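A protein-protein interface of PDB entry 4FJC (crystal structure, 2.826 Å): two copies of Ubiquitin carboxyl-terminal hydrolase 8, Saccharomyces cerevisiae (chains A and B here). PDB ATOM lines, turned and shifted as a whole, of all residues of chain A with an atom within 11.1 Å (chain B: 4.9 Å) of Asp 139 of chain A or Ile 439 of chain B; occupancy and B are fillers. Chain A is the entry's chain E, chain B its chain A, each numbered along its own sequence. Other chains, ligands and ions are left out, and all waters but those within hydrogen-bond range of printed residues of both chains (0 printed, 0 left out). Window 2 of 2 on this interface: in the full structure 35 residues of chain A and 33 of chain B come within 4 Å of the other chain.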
ATOM      1  N   VAL A 132     -22.763   5.994   4.939  1.00  0.00           N
ATOM      2  CA  VAL A 132     -21.945   6.123   3.742  1.00  0.00           C
ATOM      3  C   VAL A 132     -21.877   4.772   3.018  1.00  0.00           C
ATOM      4  O   VAL A 132     -21.740   3.733   3.661  1.00  0.00           O
ATOM      5  CB  VAL A 132     -20.518   6.630   4.112  1.00  0.00           C
ATOM      6  CG1 VAL A 132     -19.431   5.933   3.302  1.00  0.00           C
ATOM      7  CG2 VAL A 132     -20.450   8.149   3.983  1.00  0.00           C
ATOM      8  N   PRO A 133     -21.950   4.782   1.675  1.00  0.00           N
ATOM      9  CA  PRO A 133     -21.997   3.510   0.955  1.00  0.00           C
ATOM     10  C   PRO A 133     -20.714   2.674   1.085  1.00  0.00           C
ATOM     11  O   PRO A 133     -19.598   3.209   1.073  1.00  0.00           O
ATOM     12  CB  PRO A 133     -22.229   3.932  -0.508  1.00  0.00           C
ATOM     13  CG  PRO A 133     -22.469   5.413  -0.497  1.00  0.00           C
ATOM     14  CD  PRO A 133     -21.840   5.931   0.754  1.00  0.00           C
ATOM     15  N   SER A 134     -20.885   1.364   1.194  1.00  0.00           N
ATOM     16  CA  SER A 134     -19.758   0.481   1.376  1.00  0.00           C
ATOM     17  C   SER A 134     -18.781   0.580   0.209  1.00  0.00           C
ATOM     18  O   SER A 134     -19.180   0.792  -0.922  1.00  0.00           O
ATOM     19  CB  SER A 134     -20.248  -0.958   1.536  1.00  0.00           C
ATOM     20  OG  SER A 134     -20.828  -1.456   0.343  1.00  0.00           O
ATOM     21  N   MET A 135     -17.496   0.407   0.490  1.00  0.00           N
ATOM     22  CA  MET A 135     -16.467   0.385  -0.556  1.00  0.00           C
ATOM     23  C   MET A 135     -16.864  -0.533  -1.732  1.00  0.00           C
ATOM     24  O   MET A 135     -16.537  -0.259  -2.884  1.00  0.00           O
ATOM     25  CB  MET A 135     -15.147  -0.087   0.065  1.00  0.00           C
ATOM     26  CG  MET A 135     -13.923  -0.098  -0.848  1.00  0.00           C
ATOM     27  SD  MET A 135     -12.439  -0.857  -0.107  1.00  0.00           S
ATOM     28  CE  MET A 135     -13.012  -2.544   0.173  1.00  0.00           C
ATOM     29  N   GLU A 136     -17.598  -1.602  -1.427  1.00  0.00           N
ATOM     30  CA  GLU A 136     -17.851  -2.706  -2.363  1.00  0.00           C
ATOM     31  C   GLU A 136     -18.975  -2.403  -3.359  1.00  0.00           C
ATOM     32  O   GLU A 136     -18.905  -2.794  -4.518  1.00  0.00           O
ATOM     33  CB  GLU A 136     -18.220  -3.985  -1.582  1.00  0.00           C
ATOM     34  CG  GLU A 136     -17.369  -4.299  -0.342  1.00  0.00           C
ATOM     35  CD  GLU A 136     -17.986  -3.840   0.986  1.00  0.00           C
ATOM     36  OE1 GLU A 136     -17.204  -3.478   1.902  1.00  0.00           O
ATOM     37  OE2 GLU A 136     -19.232  -3.846   1.124  1.00  0.00           O
ATOM     38  N   ARG A 137     -20.008  -1.714  -2.894  1.00  0.00           N
ATOM     39  CA  ARG A 137     -21.174  -1.417  -3.714  1.00  0.00           C
ATOM     40  C   ARG A 137     -21.203   0.037  -4.203  1.00  0.00           C
ATOM     41  O   ARG A 137     -22.201   0.487  -4.753  1.00  0.00           O
ATOM     42  CB  ARG A 137     -22.451  -1.673  -2.902  1.00  0.00           C
ATOM     43  CG  ARG A 137     -22.484  -2.935  -2.052  1.00  0.00           C
ATOM     44  CD  ARG A 137     -22.890  -4.173  -2.822  1.00  0.00           C
ATOM     45  NE  ARG A 137     -21.749  -4.752  -3.526  1.00  0.00           N
ATOM     46  CZ  ARG A 137     -21.511  -4.655  -4.837  1.00  0.00           C
ATOM     47  NH1 ARG A 137     -22.333  -3.984  -5.649  1.00  0.00           N
ATOM     48  NH2 ARG A 137     -20.426  -5.235  -5.346  1.00  0.00           N
ATOM     49  N   ARG A 138     -20.114   0.771  -4.007  1.00  0.00           N
ATOM     50  CA  ARG A 138     -20.126   2.231  -4.186  1.00  0.00           C
ATOM     51  C   ARG A 138     -20.380   2.672  -5.615  1.00  0.00           C
ATOM     52  O   ARG A 138     -20.829   3.783  -5.832  1.00  0.00           O
ATOM     53  CB  ARG A 138     -18.833   2.877  -3.654  1.00  0.00           C
ATOM     54  CG  ARG A 138     -17.564   2.577  -4.443  1.00  0.00           C
ATOM     55  CD  ARG A 138     -16.384   3.345  -3.864  1.00  0.00           C
ATOM     56  NE  ARG A 138     -15.176   3.244  -4.682  1.00  0.00           N
ATOM     57  CZ  ARG A 138     -14.362   2.188  -4.722  1.00  0.00           C
ATOM     58  NH1 ARG A 138     -14.611   1.100  -4.001  1.00  0.00           N
ATOM     59  NH2 ARG A 138     -13.290   2.202  -5.508  1.00  0.00           N
ATOM     60  N   ASP A 139     -20.072   1.809  -6.579  1.00  0.00           N
ATOM     61  CA  ASP A 139     -20.356   2.057  -7.999  1.00  0.00           C
ATOM     62  C   ASP A 139     -21.349   1.050  -8.592  1.00  0.00           C
ATOM     63  O   ASP A 139     -21.537   1.020  -9.795  1.00  0.00           O
ATOM     64  CB  ASP A 139     -19.049   2.057  -8.810  1.00  0.00           C
ATOM     65  CG  ASP A 139     -18.202   3.323  -8.577  1.00  0.00           C
ATOM     66  OD1 ASP A 139     -18.776   4.436  -8.504  1.00  0.00           O
ATOM     67  OD2 ASP A 139     -16.960   3.206  -8.479  1.00  0.00           O
ATOM     68  N   GLY A 140     -22.000   0.241  -7.761  1.00  0.00           N
ATOM     69  CA  GLY A 140     -23.040  -0.684  -8.236  1.00  0.00           C
ATOM     70  C   GLY A 140     -22.560  -1.827  -9.107  1.00  0.00           C
ATOM     71  O   GLY A 140     -23.347  -2.423  -9.861  1.00  0.00           O
ATOM     72  N   LEU A 141     -21.273  -2.140  -8.987  1.00  0.00           N
ATOM     73  CA  LEU A 141     -20.663  -3.219  -9.750  1.00  0.00           C
ATOM     74  C   LEU A 141     -21.106  -4.627  -9.290  1.00  0.00           C
ATOM     75  O   LEU A 141     -20.892  -5.026  -8.141  1.00  0.00           O
ATOM     76  CB  LEU A 141     -19.140  -3.102  -9.701  1.00  0.00           C
ATOM     77  CG  LEU A 141     -18.520  -1.936 -10.476  1.00  0.00           C
ATOM     78  CD1 LEU A 141     -17.005  -1.981 -10.335  1.00  0.00           C
ATOM     79  CD2 LEU A 141     -18.917  -1.961 -11.953  1.00  0.00           C
ATOM     80  N   SER A 142     -21.738  -5.360 -10.207  1.00  0.00           N
ATOM     81  CA  SER A 142     -22.133  -6.754  -9.994  1.00  0.00           C
ATOM     82  C   SER A 142     -22.690  -7.317 -11.296  1.00  0.00           C
ATOM     83  O   SER A 142     -23.562  -6.702 -11.914  1.00  0.00           O
ATOM     84  CB  SER A 142     -23.223  -6.888  -8.921  1.00  0.00           C
ATOM     85  OG  SER A 142     -23.336  -5.712  -8.133  1.00  0.00           O
ATOM     86  N   GLY A 143     -22.190  -8.481 -11.700  1.00  0.00           N
ATOM     87  CA  GLY A 143     -22.830  -9.249 -12.751  1.00  0.00           C
ATOM     88  C   GLY A 143     -24.190  -9.797 -12.304  1.00  0.00           C
ATOM     89  O   GLY A 143     -24.546  -9.691 -11.128  1.00  0.00           O
ATOM     90  N   HIS B 162     -26.580   1.647 -14.980  1.00  0.00           N
ATOM     91  CA  HIS B 162     -25.428   2.511 -14.909  1.00  0.00           C
ATOM     92  C   HIS B 162     -25.712   3.811 -15.540  1.00  0.00           C
ATOM     93  O   HIS B 162     -24.820   4.630 -15.735  1.00  0.00           O
ATOM     94  CB  HIS B 162     -24.210   1.810 -15.426  1.00  0.00           C
ATOM     95  CG  HIS B 162     -23.634   0.877 -14.393  1.00  0.00           C
ATOM     96  ND1 HIS B 162     -23.907  -0.439 -14.367  1.00  0.00           N
ATOM     97  CD2 HIS B 162     -22.874   1.144 -13.257  1.00  0.00           C
ATOM     98  CE1 HIS B 162     -23.308  -0.992 -13.313  1.00  0.00           C
ATOM     99  NE2 HIS B 162     -22.682  -0.016 -12.628  1.00  0.00           N
ATOM    100  N   TYR B 200     -26.471  -1.293  -5.397  1.00  0.00           N
ATOM    101  CA  TYR B 200     -25.820  -0.092  -4.881  1.00  0.00           C
ATOM    102  C   TYR B 200     -25.843   0.000  -3.352  1.00  0.00           C
ATOM    103  O   TYR B 200     -24.840   0.350  -2.741  1.00  0.00           O
ATOM    104  CB  TYR B 200     -26.446   1.164  -5.512  1.00  0.00           C
ATOM    105  CG  TYR B 200     -25.902   1.520  -6.882  1.00  0.00           C
ATOM    106  CD1 TYR B 200     -24.668   2.157  -7.022  1.00  0.00           C
ATOM    107  CD2 TYR B 200     -26.627   1.248  -8.021  1.00  0.00           C
ATOM    108  CE1 TYR B 200     -24.176   2.491  -8.267  1.00  0.00           C
ATOM    109  CE2 TYR B 200     -26.149   1.585  -9.270  1.00  0.00           C
ATOM    110  CZ  TYR B 200     -24.924   2.198  -9.395  1.00  0.00           C
ATOM    111  OH  TYR B 200     -24.465   2.523 -10.656  1.00  0.00           O
ATOM    112  N   CYS B 437     -19.858  -0.346 -19.578  1.00  0.00           N
ATOM    113  CA  CYS B 437     -20.316   0.946 -19.067  1.00  0.00           C
ATOM    114  C   CYS B 437     -19.145   1.762 -18.500  1.00  0.00           C
ATOM    115  O   CYS B 437     -18.251   1.220 -17.870  1.00  0.00           O
ATOM    116  CB  CYS B 437     -21.407   0.717 -18.030  1.00  0.00           C
ATOM    117  SG  CYS B 437     -22.521  -0.632 -18.523  1.00  0.00           S
ATOM    118  N   LYS B 438     -19.137   3.059 -18.795  1.00  0.00           N
ATOM    119  CA  LYS B 438     -18.168   4.018 -18.242  1.00  0.00           C
ATOM    120  C   LYS B 438     -18.768   4.470 -16.925  1.00  0.00           C
ATOM    121  O   LYS B 438     -19.811   5.137 -16.916  1.00  0.00           O
ATOM    122  CB  LYS B 438     -18.008   5.213 -19.200  1.00  0.00           C
ATOM    123  CG  LYS B 438     -17.062   6.325 -18.769  1.00  0.00           C
ATOM    124  CD  LYS B 438     -16.879   7.388 -19.868  1.00  0.00           C
ATOM    125  CE  LYS B 438     -15.759   8.375 -19.509  1.00  0.00           C
ATOM    126  NZ  LYS B 438     -15.372   9.404 -20.531  1.00  0.00           N
ATOM    127  N   ILE B 439     -18.168   4.078 -15.807  1.00  0.00           N
ATOM    128  CA  ILE B 439     -18.726   4.486 -14.515  1.00  0.00           C
ATOM    129  C   ILE B 439     -18.088   5.776 -14.048  1.00  0.00           C
ATOM    130  O   ILE B 439     -17.048   6.207 -14.570  1.00  0.00           O
ATOM    131  CB  ILE B 439     -18.583   3.433 -13.391  1.00  0.00           C
ATOM    132  CG1 ILE B 439     -17.095   3.155 -13.101  1.00  0.00           C
ATOM    133  CG2 ILE B 439     -19.395   2.192 -13.731  1.00  0.00           C
ATOM    134  CD1 ILE B 439     -16.706   3.355 -11.651  1.00  0.00           C
ATOM    135  N   SER B 440     -18.731   6.367 -13.042  1.00  0.00           N
ATOM    136  CA  SER B 440     -18.363   7.679 -12.546  1.00  0.00           C
ATOM    137  C   SER B 440     -16.885   7.654 -12.128  1.00  0.00           C
ATOM    138  O   SER B 440     -16.469   6.800 -11.325  1.00  0.00           O
ATOM    139  CB  SER B 440     -19.314   8.081 -11.406  1.00  0.00           C
ATOM    140  OG  SER B 440     -20.678   8.105 -11.844  1.00  0.00           O
ATOM    141  N   GLY B 441     -16.105   8.561 -12.725  1.00  0.00           N
ATOM    142  CA  GLY B 441     -14.645   8.544 -12.618  1.00  0.00           C
ATOM    143  C   GLY B 441     -13.961   8.540 -13.973  1.00  0.00           C
ATOM    144  O   GLY B 441     -12.973   9.238 -14.169  1.00  0.00           O
ATOM    145  N   GLY B 442     -14.490   7.763 -14.920  1.00  0.00           N
ATOM    146  CA  GLY B 442     -13.892   7.634 -16.263  1.00  0.00           C
ATOM    147  C   GLY B 442     -13.382   6.239 -16.578  1.00  0.00           C
ATOM    148  O   GLY B 442     -12.845   5.985 -17.664  1.00  0.00           O
ATOM    149  N   GLN B 443     -13.578   5.341 -15.615  1.00  0.00           N
ATOM    150  CA  GLN B 443     -13.116   3.950 -15.667  1.00  0.00           C
ATOM    151  C   GLN B 443     -14.184   2.992 -16.254  1.00  0.00           C
ATOM    152  O   GLN B 443     -15.329   2.937 -15.779  1.00  0.00           O
ATOM    153  CB  GLN B 443     -12.680   3.496 -14.253  1.00  0.00           C
ATOM    154  CG  GLN B 443     -13.725   3.710 -13.144  1.00  0.00           C
ATOM    155  CD  GLN B 443     -13.139   3.953 -11.743  1.00  0.00           C
ATOM    156  OE1 GLN B 443     -13.155   5.084 -11.237  1.00  0.00           O
ATOM    157  NE2 GLN B 443     -12.643   2.887 -11.103  1.00  0.00           N
ATOM    158  N   PHE B 445     -15.870  -0.637 -17.311  1.00  0.00           N
ATOM    159  CA  PHE B 445     -16.039  -2.026 -16.935  1.00  0.00           C
ATOM    160  C   PHE B 445     -16.788  -2.848 -17.996  1.00  0.00           C
ATOM    161  O   PHE B 445     -17.452  -2.312 -18.862  1.00  0.00           O
ATOM    162  CB  PHE B 445     -16.741  -2.094 -15.582  1.00  0.00           C
ATOM    163  CG  PHE B 445     -15.886  -1.593 -14.458  1.00  0.00           C
ATOM    164  CD1 PHE B 445     -15.839  -0.242 -14.154  1.00  0.00           C
ATOM    165  CD2 PHE B 445     -15.084  -2.464 -13.742  1.00  0.00           C
ATOM    166  CE1 PHE B 445     -15.026   0.232 -13.135  1.00  0.00           C
ATOM    167  CE2 PHE B 445     -14.273  -1.997 -12.721  1.00  0.00           C
ATOM    168  CZ  PHE B 445     -14.244  -0.644 -12.421  1.00  0.00           C
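The backbone carbonyl oxygen (O) of Asp 139 of chain A sits at hydrogen-bond distance from a ring nitrogen (NE2) of His 162 of chain B, 3.2 Å away. The side-chain hydroxyl (OH) of Tyr 200 of chain B sits close to the backbone carbonyl oxygen (O) of Asp 139 of chain A (3.4 Å). The backbone carbonyl oxygen of Tyr 200 of chain B lies close to the backbone carbonyl oxygen of Arg 137 of chain A.
The backbone NH of Phe 445 of chain B lies within hydrogen-bond range of the backbone carbonyl oxygen of Cys 437 of chain B, 3.1 Å away. N of Arg 137 of chain A lies close to OG of Ser 134 of chain A (3.3 Å). NH2 of Arg 137 of chain A sits at hydrogen-bond distance from O of Leu 141 of chain A (2.8 Å). OG of Ser 142 of chain A sits at hydrogen-bond distance from NH1 of Arg 137 of chain A, at 3.2 Å.
CD1 of Ile 439 of chain B touches OD2 of Asp 139 of chain A, 3.2 Å away. Gly 140 of chain A touches His 162 of chain B. Gly 140 of chain A touches Tyr 200 of chain B. Phe 445 of chain B touches Leu 141 of chain A (CE2 to CD1, 3.6 Å).
Of the printed residues of chain B, Arg 137 of chain A touches Tyr 200 (3.1 Å). Arg 138 of chain A touches none of the printed residues of chain B. Of chain B, only His 162, Tyr 200 and Ile 439 come within 4 Å of Asp 139 of chain A. Ser 142 of chain A touches none of the printed residues of chain B. Of chain A, only Arg 137 (3.1 Å), Asp 139 (3.2 Å) and Gly 140 (3.2 Å) come within 4 Å of Tyr 200 of chain B. No residue of chain A comes within 4 Å of Cys 437 of chain B. No residue of chain A comes within 4 Å of Lys 438 of chain B. Ile 439 of chain B touches one residue of chain A. No residue of chain A comes within 4 Å of Ser 440 of chain B. No residue of chain A comes within 4 Å of Gly 441 of chain B. Of the printed residues of chain A, Phe 445 of chain B touches Leu 141 (3.6 Å). The nearest residue of chain A that does not touch Ile 439 of chain B is Leu 141 of chain A (4.5 Å). The nearest printed residue of chain A that does not touch Phe 445 of chain B is Asp 139 of chain A (5.9 Å).
Printed residues of chain A that touch a printed residue of chain B: Arg 137, Asp 139, Gly 140 and Leu 141. Hydrophobic or aromatic side chains of chain A within 4 Å of the printed part of chain B: Leu 141. Of the 10 printed residues of chain B, 4 touch a printed residue of chain A. Hydrophobic or aromatic side chains of chain B that line the printed part of chain A: His 162, Tyr 200, Ile 439 and Phe 445. Among the printed residues, no Asp or Glu carboxylate lies within 4 Å of a Lys or Arg side-chain nitrogen of the other chain.
No position is printed for both chains.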
